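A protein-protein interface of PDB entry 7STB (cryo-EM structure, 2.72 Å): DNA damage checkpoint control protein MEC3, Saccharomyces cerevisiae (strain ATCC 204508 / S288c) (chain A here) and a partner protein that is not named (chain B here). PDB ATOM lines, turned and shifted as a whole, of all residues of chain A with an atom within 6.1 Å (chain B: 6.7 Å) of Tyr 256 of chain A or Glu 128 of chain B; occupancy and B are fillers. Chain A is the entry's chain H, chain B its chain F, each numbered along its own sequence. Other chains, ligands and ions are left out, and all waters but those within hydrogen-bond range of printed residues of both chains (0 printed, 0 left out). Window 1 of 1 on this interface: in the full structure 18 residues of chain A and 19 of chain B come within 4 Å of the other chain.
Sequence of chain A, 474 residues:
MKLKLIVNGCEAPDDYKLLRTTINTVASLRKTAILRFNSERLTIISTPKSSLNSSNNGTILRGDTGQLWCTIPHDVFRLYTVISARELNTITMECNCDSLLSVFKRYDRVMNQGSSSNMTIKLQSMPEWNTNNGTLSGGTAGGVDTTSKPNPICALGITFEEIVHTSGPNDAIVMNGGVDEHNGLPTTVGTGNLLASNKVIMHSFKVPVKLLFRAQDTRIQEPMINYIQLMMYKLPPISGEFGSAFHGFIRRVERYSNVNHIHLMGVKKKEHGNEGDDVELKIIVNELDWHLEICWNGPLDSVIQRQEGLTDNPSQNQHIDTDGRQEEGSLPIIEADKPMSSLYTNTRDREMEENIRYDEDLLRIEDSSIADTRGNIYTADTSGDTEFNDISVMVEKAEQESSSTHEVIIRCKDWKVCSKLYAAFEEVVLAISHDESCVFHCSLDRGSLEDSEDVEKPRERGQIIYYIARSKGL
Val 253 of chain A touches none of the printed residues of chain B. Of the printed residues of chain B, Ser 257 of chain A touches His 88 (3.97 Å) and Asp 91 (2.9 Å). Leu 119 of chain B touches none of the printed residues of chain A. Of the printed residues of chain A, Ser 127 of chain B touches Ile 294 (3.8 Å) and Cys 295 (3.0 Å). Glu 128 of chain B touches four residues of chain A. Of the printed residues of chain A, Arg 129 of chain B touches Glu 293. Of the printed residues of chain A, Val 130 of chain B touches Leu 292. The nearest residue of chain B that does not touch Tyr 256 of chain A is Asp 91 of chain B (4.7 Å). The nearest residue of chain A that does not touch Glu 128 of chain B is Arg 252 of chain A (4.4 Å).
Among the printed residues, pairs that only touch across the chains: Arg 252 of chain A with Ile 126 of chain B (3.8 Å), Tyr 256 of chain A with His 88 of chain B (3.4 Å), Tyr 256 of chain A with Ser 92 of chain B (3.7 Å), Tyr 256 of chain A with Glu 128 of chain B (3.9 Å), Ser 257 of chain A with His 88 of chain B (3.97 Å), Trp 290 of chain A with His 88 of chain B (3.1 Å), Trp 290 of chain A with Ser 92 of chain B (3.6 Å), Trp 290 of chain A with Tyr 132 of chain B (2.9 Å), Leu 292 of chain A with Glu 128 of chain B (2.8 Å), Leu 292 of chain A with Val 130 of chain B (3.3 Å), Ile 294 of chain A with Ser 127 of chain B (3.8 Å), Ile 294 of chain A with Glu 128 of chain B (3.0 Å) and Cys 295 of chain A with Ile 126 of chain B (3.7 Å).
Of the 15 printed residues of chain B, 10 touch a printed residue of chain A. Of the 15 printed residues of chain A, 10 touch a printed residue of chain B. Hydrophobic or aromatic side chains of chain A within 4 Å of the printed part of chain B: Tyr 256, Trp 290, Leu 292 and Ile 294. Among the printed residues, 21 pairs touch across the chains. Among the printed residues, Asp or Glu carboxylates within 4 Å of a Lys or Arg side-chain nitrogen of the other chain: Arg 252 of chain A with Asp 123 of chain B (3.1 Å).
N of Arg 129 of chain B lies within hydrogen-bond range of O of Glu 293 of chain A, at 3.3 Å. The side-chain amide oxygen (OD1) of Asn 258 of chain A lies within hydrogen-bond range of a ring nitrogen (ND1) of His 88 of chain B (2.8 Å). The guanidinium group (NH1) of Arg 255 of chain A lies close to the backbone carbonyl oxygen (O) of Asp 91 of chain B (2.2 Å). The backbone carbonyl oxygen of Ser 127 of chain B sits at hydrogen-bond distance from the backbone NH of Cys 295 of chain A, 3.0 Å away. The side-chain carboxylate (OD2) of Asp 123 of chain B lies within salt-bridge range of the guanidinium group (NH2) of Arg 252 of chain A (3.1 Å). The guanidinium group (NH1) of Arg 255 of chain A sits at hydrogen-bond distance from the backbone carbonyl oxygen (O) of Ser 92 of chain B (2.9 Å). O of Glu 293 of chain A sits close to OE2 of Glu 128 of chain B (3.1 Å). The side-chain carboxylate (OD2) of Asp 91 of chain B is in hydrogen-bond range of the side-chain hydroxyl (OG) of Ser 257 of chain A.
The guanidinium group of Arg 255 of chain A sits at hydrogen-bond distance from the side-chain hydroxyl of Tyr 256 of chain A, at 3.1 Å. OH of Tyr 132 of chain B is in hydrogen-bond range of OG of Ser 92 of chain B, 3.0 Å away. N of Phe 121 of chain B lies within hydrogen-bond range of O of Glu 128 of chain B (2.9 Å). SG of Cys 295 of chain A sits at hydrogen-bond distance from OE2 of Glu 293 of chain A (2.8 Å). O of Ile 283 of chain A is in hydrogen-bond range of N of Ile 294 of chain A, 2.8 Å away. The backbone carbonyl oxygen of Leu 119 of chain B lies within hydrogen-bond range of the backbone NH of Val 130 of chain B, at 2.9 Å.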
ATOM      1  N   ARG A 252     -12.905 -16.186   8.203  1.00  0.00           N
ATOM      2  CA  ARG A 252     -11.495 -16.570   8.216  1.00  0.00           C
ATOM      3  C   ARG A 252     -10.896 -16.493   9.615  1.00  0.00           C
ATOM      4  O   ARG A 252     -10.145 -17.385  10.026  1.00  0.00           O
ATOM      5  CB  ARG A 252     -10.687 -15.679   7.266  1.00  0.00           C
ATOM      6  CG  ARG A 252     -10.888 -15.937   5.776  1.00  0.00           C
ATOM      7  CD  ARG A 252     -10.688 -17.397   5.396  1.00  0.00           C
ATOM      8  NE  ARG A 252     -10.813 -17.608   3.958  1.00  0.00           N
ATOM      9  CZ  ARG A 252     -11.010 -18.788   3.386  1.00  0.00           C
ATOM     10  NH1 ARG A 252     -11.116 -19.895   4.103  1.00  0.00           N
ATOM     11  NH2 ARG A 252     -11.104 -18.860   2.062  1.00  0.00           N
ATOM     12  N   VAL A 253     -11.207 -15.429  10.363  1.00  0.00           N
ATOM     13  CA  VAL A 253     -10.564 -15.200  11.654  1.00  0.00           C
ATOM     14  C   VAL A 253     -11.270 -15.912  12.799  1.00  0.00           C
ATOM     15  O   VAL A 253     -10.801 -15.843  13.943  1.00  0.00           O
ATOM     16  CB  VAL A 253     -10.478 -13.688  11.950  1.00  0.00           C
ATOM     17  CG1 VAL A 253      -9.527 -13.419  13.111  1.00  0.00           C
ATOM     18  CG2 VAL A 253     -10.040 -12.935  10.703  1.00  0.00           C
ATOM     19  N   GLU A 254     -12.376 -16.607  12.532  1.00  0.00           N
ATOM     20  CA  GLU A 254     -13.120 -17.318  13.561  1.00  0.00           C
ATOM     21  C   GLU A 254     -12.641 -18.753  13.749  1.00  0.00           C
ATOM     22  O   GLU A 254     -13.421 -19.605  14.192  1.00  0.00           O
ATOM     23  CB  GLU A 254     -14.615 -17.308  13.232  1.00  0.00           C
ATOM     24  CG  GLU A 254     -15.195 -15.919  13.034  1.00  0.00           C
ATOM     25  CD  GLU A 254     -16.665 -15.951  12.665  1.00  0.00           C
ATOM     26  OE1 GLU A 254     -17.239 -17.058  12.602  1.00  0.00           O
ATOM     27  OE2 GLU A 254     -17.244 -14.869  12.439  1.00  0.00           O
ATOM     28  N   ARG A 255     -11.379 -19.041  13.420  1.00  0.00           N
ATOM     29  CA  ARG A 255     -10.828 -20.383  13.563  1.00  0.00           C
ATOM     30  C   ARG A 255      -9.440 -20.385  14.195  1.00  0.00           C
ATOM     31  O   ARG A 255      -8.740 -21.400  14.112  1.00  0.00           O
ATOM     32  CB  ARG A 255     -10.783 -21.085  12.200  1.00  0.00           C
ATOM     33  CG  ARG A 255      -9.842 -20.437  11.200  1.00  0.00           C
ATOM     34  CD  ARG A 255      -9.819 -21.192   9.881  1.00  0.00           C
ATOM     35  NE  ARG A 255      -8.980 -20.527   8.892  1.00  0.00           N
ATOM     36  CZ  ARG A 255      -7.675 -20.724   8.755  1.00  0.00           C
ATOM     37  NH1 ARG A 255      -7.017 -21.565   9.536  1.00  0.00           N
ATOM     38  NH2 ARG A 255      -7.015 -20.059   7.812  1.00  0.00           N
ATOM     39  N   TYR A 256      -9.026 -19.287  14.821  1.00  0.00           N
ATOM     40  CA  TYR A 256      -7.740 -19.196  15.501  1.00  0.00           C
ATOM     41  C   TYR A 256      -7.972 -19.201  17.006  1.00  0.00           C
ATOM     42  O   TYR A 256      -8.800 -18.437  17.514  1.00  0.00           O
ATOM     43  CB  TYR A 256      -6.987 -17.936  15.074  1.00  0.00           C
ATOM     44  CG  TYR A 256      -6.728 -17.862  13.586  1.00  0.00           C
ATOM     45  CD1 TYR A 256      -5.677 -18.560  13.009  1.00  0.00           C
ATOM     46  CD2 TYR A 256      -7.536 -17.097  12.757  1.00  0.00           C
ATOM     47  CE1 TYR A 256      -5.436 -18.498  11.651  1.00  0.00           C
ATOM     48  CE2 TYR A 256      -7.303 -17.029  11.397  1.00  0.00           C
ATOM     49  CZ  TYR A 256      -6.251 -17.732  10.849  1.00  0.00           C
ATOM     50  OH  TYR A 256      -6.011 -17.669   9.496  1.00  0.00           O
ATOM     51  N   SER A 257      -7.239 -20.061  17.713  1.00  0.00           N
ATOM     52  CA  SER A 257      -7.503 -20.324  19.124  1.00  0.00           C
ATOM     53  C   SER A 257      -7.313 -19.093  20.005  1.00  0.00           C
ATOM     54  O   SER A 257      -8.276 -18.596  20.597  1.00  0.00           O
ATOM     55  CB  SER A 257      -6.598 -21.454  19.619  1.00  0.00           C
ATOM     56  OG  SER A 257      -6.721 -22.601  18.797  1.00  0.00           O
ATOM     57  N   ASN A 258      -6.080 -18.591  20.097  1.00  0.00           N
ATOM     58  CA  ASN A 258      -5.762 -17.549  21.068  1.00  0.00           C
ATOM     59  C   ASN A 258      -6.167 -16.155  20.611  1.00  0.00           C
ATOM     60  O   ASN A 258      -6.089 -15.216  21.410  1.00  0.00           O
ATOM     61  CB  ASN A 258      -4.263 -17.561  21.380  1.00  0.00           C
ATOM     62  CG  ASN A 258      -3.411 -17.223  20.171  1.00  0.00           C
ATOM     63  OD1 ASN A 258      -3.927 -16.857  19.117  1.00  0.00           O
ATOM     64  ND2 ASN A 258      -2.097 -17.342  20.322  1.00  0.00           N
ATOM     65  N   VAL A 259      -6.588 -15.991  19.357  1.00  0.00           N
ATOM     66  CA  VAL A 259      -6.960 -14.672  18.863  1.00  0.00           C
ATOM     67  C   VAL A 259      -8.230 -14.214  19.565  1.00  0.00           C
ATOM     68  O   VAL A 259      -9.227 -14.945  19.620  1.00  0.00           O
ATOM     69  CB  VAL A 259      -7.140 -14.701  17.338  1.00  0.00           C
ATOM     70  CG1 VAL A 259      -7.679 -13.370  16.837  1.00  0.00           C
ATOM     71  CG2 VAL A 259      -5.822 -15.041  16.657  1.00  0.00           C
ATOM     72  N   ASN A 260      -8.194 -13.000  20.116  1.00  0.00           N
ATOM     73  CA  ASN A 260      -9.334 -12.459  20.845  1.00  0.00           C
ATOM     74  C   ASN A 260      -9.673 -11.046  20.386  1.00  0.00           C
ATOM     75  O   ASN A 260     -10.828 -10.620  20.479  1.00  0.00           O
ATOM     76  CB  ASN A 260      -9.050 -12.469  22.348  1.00  0.00           C
ATOM     77  CG  ASN A 260      -7.878 -11.584  22.724  1.00  0.00           C
ATOM     78  OD1 ASN A 260      -6.791 -11.701  22.157  1.00  0.00           O
ATOM     79  ND2 ASN A 260      -8.091 -10.694  23.686  1.00  0.00           N
ATOM     80  N   ILE A 283      -8.392  -7.460   7.615  1.00  0.00           N
ATOM     81  CA  ILE A 283      -8.469  -7.888   9.008  1.00  0.00           C
ATOM     82  C   ILE A 283      -7.079  -8.316   9.452  1.00  0.00           C
ATOM     83  O   ILE A 283      -6.437  -9.134   8.787  1.00  0.00           O
ATOM     84  CB  ILE A 283      -9.479  -9.034   9.200  1.00  0.00           C
ATOM     85  CG1 ILE A 283     -10.849  -8.644   8.638  1.00  0.00           C
ATOM     86  CG2 ILE A 283      -9.595  -9.386  10.675  1.00  0.00           C
ATOM     87  CD1 ILE A 283     -11.822  -9.802   8.531  1.00  0.00           C
ATOM     88  N   TRP A 290       2.955 -13.690  16.289  1.00  0.00           N
ATOM     89  CA  TRP A 290       2.042 -13.954  15.190  1.00  0.00           C
ATOM     90  C   TRP A 290       1.768 -12.675  14.414  1.00  0.00           C
ATOM     91  O   TRP A 290       1.793 -11.573  14.970  1.00  0.00           O
ATOM     92  CB  TRP A 290       0.721 -14.538  15.704  1.00  0.00           C
ATOM     93  CG  TRP A 290      -0.057 -15.270  14.665  1.00  0.00           C
ATOM     94  CD1 TRP A 290      -0.801 -14.723  13.661  1.00  0.00           C
ATOM     95  CD2 TRP A 290      -0.173 -16.690  14.522  1.00  0.00           C
ATOM     96  NE1 TRP A 290      -1.372 -15.715  12.901  1.00  0.00           N
ATOM     97  CE2 TRP A 290      -1.002 -16.931  13.410  1.00  0.00           C
ATOM     98  CE3 TRP A 290       0.344 -17.780  15.228  1.00  0.00           C
ATOM     99  CZ2 TRP A 290      -1.326 -18.215  12.988  1.00  0.00           C
ATOM    100  CZ3 TRP A 290       0.019 -19.054  14.808  1.00  0.00           C
ATOM    101  CH2 TRP A 290      -0.807 -19.261  13.697  1.00  0.00           C
ATOM    102  N   LEU A 292      -1.169 -12.143  11.553  1.00  0.00           N
ATOM    103  CA  LEU A 292      -2.242 -12.568  10.665  1.00  0.00           C
ATOM    104  C   LEU A 292      -2.759 -11.363   9.892  1.00  0.00           C
ATOM    105  O   LEU A 292      -2.933 -10.284  10.462  1.00  0.00           O
ATOM    106  CB  LEU A 292      -3.385 -13.202  11.459  1.00  0.00           C
ATOM    107  CG  LEU A 292      -4.567 -13.759  10.666  1.00  0.00           C
ATOM    108  CD1 LEU A 292      -4.127 -14.911   9.789  1.00  0.00           C
ATOM    109  CD2 LEU A 292      -5.685 -14.188  11.601  1.00  0.00           C
ATOM    110  N   GLU A 293      -3.014 -11.551   8.599  1.00  0.00           N
ATOM    111  CA  GLU A 293      -3.475 -10.444   7.766  1.00  0.00           C
ATOM    112  C   GLU A 293      -4.289 -11.010   6.613  1.00  0.00           C
ATOM    113  O   GLU A 293      -3.770 -11.805   5.822  1.00  0.00           O
ATOM    114  CB  GLU A 293      -2.285  -9.630   7.256  1.00  0.00           C
ATOM    115  CG  GLU A 293      -2.658  -8.322   6.582  1.00  0.00           C
ATOM    116  CD  GLU A 293      -3.037  -8.484   5.129  1.00  0.00           C
ATOM    117  OE1 GLU A 293      -2.534  -9.422   4.474  1.00  0.00           O
ATOM    118  OE2 GLU A 293      -3.840  -7.663   4.643  1.00  0.00           O
ATOM    119  N   ILE A 294      -5.553 -10.605   6.519  1.00  0.00           N
ATOM    120  CA  ILE A 294      -6.488 -11.096   5.515  1.00  0.00           C
ATOM    121  C   ILE A 294      -6.939  -9.911   4.675  1.00  0.00           C
ATOM    122  O   ILE A 294      -7.409  -8.904   5.220  1.00  0.00           O
ATOM    123  CB  ILE A 294      -7.707 -11.787   6.155  1.00  0.00           C
ATOM    124  CG1 ILE A 294      -7.260 -12.797   7.209  1.00  0.00           C
ATOM    125  CG2 ILE A 294      -8.527 -12.510   5.098  1.00  0.00           C
ATOM    126  CD1 ILE A 294      -7.234 -12.245   8.617  1.00  0.00           C
ATOM    127  N   CYS A 295      -6.805 -10.040   3.356  1.00  0.00           N
ATOM    128  CA  CYS A 295      -7.241  -9.038   2.395  1.00  0.00           C
ATOM    129  C   CYS A 295      -8.516  -9.499   1.702  1.00  0.00           C
ATOM    130  O   CYS A 295      -8.830 -10.691   1.653  1.00  0.00           O
ATOM    131  CB  CYS A 295      -6.165  -8.776   1.334  1.00  0.00           C
ATOM    132  SG  CYS A 295      -4.584  -8.185   1.958  1.00  0.00           S
ATOM    133  N   HIS B  88      -1.045 -21.410  17.784  1.00  0.00           N
ATOM    134  CA  HIS B  88      -2.209 -21.959  17.099  1.00  0.00           C
ATOM    135  C   HIS B  88      -1.910 -22.230  15.628  1.00  0.00           C
ATOM    136  O   HIS B  88      -2.810 -22.149  14.784  1.00  0.00           O
ATOM    137  CB  HIS B  88      -3.414 -21.026  17.239  1.00  0.00           C
ATOM    138  CG  HIS B  88      -3.168 -19.640  16.731  1.00  0.00           C
ATOM    139  ND1 HIS B  88      -2.555 -18.666  17.489  1.00  0.00           N
ATOM    140  CD2 HIS B  88      -3.465 -19.062  15.544  1.00  0.00           C
ATOM    141  CE1 HIS B  88      -2.476 -17.550  16.787  1.00  0.00           C
ATOM    142  NE2 HIS B  88      -3.022 -17.763  15.604  1.00  0.00           N
ATOM    143  N   ASP B  91      -4.248 -24.608  13.524  1.00  0.00           N
ATOM    144  CA  ASP B  91      -5.474 -24.125  12.902  1.00  0.00           C
ATOM    145  C   ASP B  91      -5.198 -23.225  11.702  1.00  0.00           C
ATOM    146  O   ASP B  91      -6.032 -23.142  10.795  1.00  0.00           O
ATOM    147  CB  ASP B  91      -6.320 -23.373  13.930  1.00  0.00           C
ATOM    148  CG  ASP B  91      -6.814 -24.271  15.047  1.00  0.00           C
ATOM    149  OD1 ASP B  91      -7.007 -25.479  14.799  1.00  0.00           O
ATOM    150  OD2 ASP B  91      -7.007 -23.768  16.173  1.00  0.00           O
ATOM    151  N   SER B  92      -4.047 -22.548  11.679  1.00  0.00           N
ATOM    152  CA  SER B  92      -3.764 -21.613  10.594  1.00  0.00           C
ATOM    153  C   SER B  92      -3.776 -22.319   9.244  1.00  0.00           C
ATOM    154  O   SER B  92      -4.458 -21.883   8.309  1.00  0.00           O
ATOM    155  CB  SER B  92      -2.417 -20.929  10.831  1.00  0.00           C
ATOM    156  OG  SER B  92      -2.114 -20.030   9.779  1.00  0.00           O
ATOM    157  N   VAL B  93      -3.026 -23.410   9.122  1.00  0.00           N
ATOM    158  CA  VAL B  93      -3.044 -24.225   7.894  1.00  0.00           C
ATOM    159  C   VAL B  93      -4.115 -25.286   8.113  1.00  0.00           C
ATOM    160  O   VAL B  93      -3.855 -26.417   8.532  1.00  0.00           O
ATOM    161  CB  VAL B  93      -1.670 -24.820   7.573  1.00  0.00           C
ATOM    162  CG1 VAL B  93      -1.719 -25.595   6.263  1.00  0.00           C
ATOM    163  CG2 VAL B  93      -0.619 -23.724   7.506  1.00  0.00           C
ATOM    164  N   LEU B 119       3.562 -18.082   5.178  1.00  0.00           N
ATOM    165  CA  LEU B 119       2.607 -18.961   4.512  1.00  0.00           C
ATOM    166  C   LEU B 119       1.523 -18.095   3.890  1.00  0.00           C
ATOM    167  O   LEU B 119       0.881 -17.303   4.589  1.00  0.00           O
ATOM    168  CB  LEU B 119       2.000 -19.971   5.487  1.00  0.00           C
ATOM    169  CG  LEU B 119       2.959 -20.992   6.103  1.00  0.00           C
ATOM    170  CD1 LEU B 119       3.791 -20.369   7.213  1.00  0.00           C
ATOM    171  CD2 LEU B 119       2.185 -22.192   6.623  1.00  0.00           C
ATOM    172  N   ILE B 120       1.322 -18.242   2.582  1.00  0.00           N
ATOM    173  CA  ILE B 120       0.378 -17.424   1.832  1.00  0.00           C
ATOM    174  C   ILE B 120      -0.630 -18.337   1.150  1.00  0.00           C
ATOM    175  O   ILE B 120      -0.251 -19.291   0.460  1.00  0.00           O
ATOM    176  CB  ILE B 120       1.089 -16.527   0.803  1.00  0.00           C
ATOM    177  CG1 ILE B 120       1.966 -15.493   1.512  1.00  0.00           C
ATOM    178  CG2 ILE B 120       0.076 -15.836  -0.098  1.00  0.00           C
ATOM    179  CD1 ILE B 120       3.128 -15.007   0.675  1.00  0.00           C
ATOM    180  N   PHE B 121      -1.911 -18.041   1.353  1.00  0.00           N
ATOM    181  CA  PHE B 121      -3.013 -18.731   0.697  1.00  0.00           C
ATOM    182  C   PHE B 121      -3.605 -17.784  -0.339  1.00  0.00           C
ATOM    183  O   PHE B 121      -3.964 -16.647  -0.011  1.00  0.00           O
ATOM    184  CB  PHE B 121      -4.092 -19.152   1.698  1.00  0.00           C
ATOM    185  CG  PHE B 121      -3.674 -20.250   2.643  1.00  0.00           C
ATOM    186  CD1 PHE B 121      -2.357 -20.673   2.725  1.00  0.00           C
ATOM    187  CD2 PHE B 121      -4.613 -20.855   3.462  1.00  0.00           C
ATOM    188  CE1 PHE B 121      -1.991 -21.675   3.602  1.00  0.00           C
ATOM    189  CE2 PHE B 121      -4.250 -21.858   4.337  1.00  0.00           C
ATOM    190  CZ  PHE B 121      -2.937 -22.269   4.407  1.00  0.00           C
ATOM    191  N   GLU B 122      -3.705 -18.251  -1.579  1.00  0.00           N
ATOM    192  CA  GLU B 122      -4.269 -17.475  -2.674  1.00  0.00           C
ATOM    193  C   GLU B 122      -5.566 -18.126  -3.132  1.00  0.00           C
ATOM    194  O   GLU B 122      -5.585 -19.316  -3.467  1.00  0.00           O
ATOM    195  CB  GLU B 122      -3.284 -17.374  -3.841  1.00  0.00           C
ATOM    196  CG  GLU B 122      -1.898 -16.888  -3.444  1.00  0.00           C
ATOM    197  CD  GLU B 122      -0.908 -16.946  -4.591  1.00  0.00           C
ATOM    198  OE1 GLU B 122      -1.348 -17.098  -5.750  1.00  0.00           O
ATOM    199  OE2 GLU B 122       0.310 -16.839  -4.334  1.00  0.00           O
ATOM    200  N   ASP B 123      -6.640 -17.345  -3.137  1.00  0.00           N
ATOM    201  CA  ASP B 123      -7.959 -17.780  -3.576  1.00  0.00           C
ATOM    202  C   ASP B 123      -8.408 -16.911  -4.749  1.00  0.00           C
ATOM    203  O   ASP B 123      -7.646 -16.093  -5.273  1.00  0.00           O
ATOM    204  CB  ASP B 123      -8.958 -17.720  -2.418  1.00  0.00           C
ATOM    205  CG  ASP B 123      -8.441 -18.392  -1.162  1.00  0.00           C
ATOM    206  OD1 ASP B 123      -7.472 -19.171  -1.257  1.00  0.00           O
ATOM    207  OD2 ASP B 123      -9.006 -18.138  -0.077  1.00  0.00           O
ATOM    208  N   ILE B 126      -9.664 -13.869  -2.154  1.00  0.00           N
ATOM    209  CA  ILE B 126      -9.170 -13.741  -0.787  1.00  0.00           C
ATOM    210  C   ILE B 126      -7.686 -14.076  -0.780  1.00  0.00           C
ATOM    211  O   ILE B 126      -7.274 -15.106  -1.327  1.00  0.00           O
ATOM    212  CB  ILE B 126      -9.938 -14.654   0.187  1.00  0.00           C
ATOM    213  CG1 ILE B 126     -11.449 -14.514  -0.023  1.00  0.00           C
ATOM    214  CG2 ILE B 126      -9.566 -14.322   1.626  1.00  0.00           C
ATOM    215  CD1 ILE B 126     -12.277 -15.439   0.845  1.00  0.00           C
ATOM    216  N   SER B 127      -6.888 -13.208  -0.159  1.00  0.00           N
ATOM    217  CA  SER B 127      -5.445 -13.394  -0.042  1.00  0.00           C
ATOM    218  C   SER B 127      -5.079 -13.399   1.437  1.00  0.00           C
ATOM    219  O   SER B 127      -5.330 -12.419   2.147  1.00  0.00           O
ATOM    220  CB  SER B 127      -4.688 -12.297  -0.790  1.00  0.00           C
ATOM    221  OG  SER B 127      -3.288 -12.459  -0.650  1.00  0.00           O
ATOM    222  N   GLU B 128      -4.489 -14.499   1.897  1.00  0.00           N
ATOM    223  CA  GLU B 128      -4.054 -14.658   3.276  1.00  0.00           C
ATOM    224  C   GLU B 128      -2.536 -14.739   3.336  1.00  0.00           C
ATOM    225  O   GLU B 128      -1.914 -15.410   2.511  1.00  0.00           O
ATOM    226  CB  GLU B 128      -4.662 -15.920   3.894  1.00  0.00           C
ATOM    227  CG  GLU B 128      -4.335 -16.134   5.362  1.00  0.00           C
ATOM    228  CD  GLU B 128      -5.202 -15.319   6.284  1.00  0.00           C
ATOM    229  OE1 GLU B 128      -6.437 -15.505   6.270  1.00  0.00           O
ATOM    230  OE2 GLU B 128      -4.641 -14.493   7.029  1.00  0.00           O
ATOM    231  N   ARG B 129      -1.949 -14.062   4.320  1.00  0.00           N
ATOM    232  CA  ARG B 129      -0.520 -14.159   4.586  1.00  0.00           C
ATOM    233  C   ARG B 129      -0.308 -14.212   6.090  1.00  0.00           C
ATOM    234  O   ARG B 129      -0.857 -13.386   6.823  1.00  0.00           O
ATOM    235  CB  ARG B 129       0.246 -12.977   3.982  1.00  0.00           C
ATOM    236  CG  ARG B 129       1.707 -12.915   4.400  1.00  0.00           C
ATOM    237  CD  ARG B 129       2.493 -11.916   3.569  1.00  0.00           C
ATOM    238  NE  ARG B 129       3.864 -11.776   4.047  1.00  0.00           N
ATOM    239  CZ  ARG B 129       4.807 -11.076   3.431  1.00  0.00           C
ATOM    240  NH1 ARG B 129       4.565 -10.432   2.301  1.00  0.00           N
ATOM    241  NH2 ARG B 129       6.025 -11.021   3.964  1.00  0.00           N
ATOM    242  N   VAL B 130       0.484 -15.180   6.545  1.00  0.00           N
ATOM    243  CA  VAL B 130       0.812 -15.331   7.959  1.00  0.00           C
ATOM    244  C   VAL B 130       2.320 -15.469   8.093  1.00  0.00           C
ATOM    245  O   VAL B 130       2.950 -16.226   7.345  1.00  0.00           O
ATOM    246  CB  VAL B 130       0.097 -16.540   8.594  1.00  0.00           C
ATOM    247  CG1 VAL B 130      -1.394 -16.289   8.671  1.00  0.00           C
ATOM    248  CG2 VAL B 130       0.385 -17.808   7.816  1.00  0.00           C
ATOM    249  N   TYR B 132       5.572 -16.227  10.760  1.00  0.00           N
ATOM    250  CA  TYR B 132       5.979 -16.848  12.013  1.00  0.00           C
ATOM    251  C   TYR B 132       7.430 -16.488  12.298  1.00  0.00           C
ATOM    252  O   TYR B 132       8.300 -16.684  11.444  1.00  0.00           O
ATOM    253  CB  TYR B 132       5.821 -18.368  11.951  1.00  0.00           C
ATOM    254  CG  TYR B 132       4.399 -18.835  11.756  1.00  0.00           C
ATOM    255  CD1 TYR B 132       3.791 -18.766  10.510  1.00  0.00           C
ATOM    256  CD2 TYR B 132       3.670 -19.359  12.813  1.00  0.00           C
ATOM    257  CE1 TYR B 132       2.492 -19.196  10.326  1.00  0.00           C
ATOM    258  CE2 TYR B 132       2.371 -19.791  12.638  1.00  0.00           C
ATOM    259  CZ  TYR B 132       1.787 -19.708  11.393  1.00  0.00           C
ATOM    260  OH  TYR B 132       0.495 -20.139  11.210  1.00  0.00           O
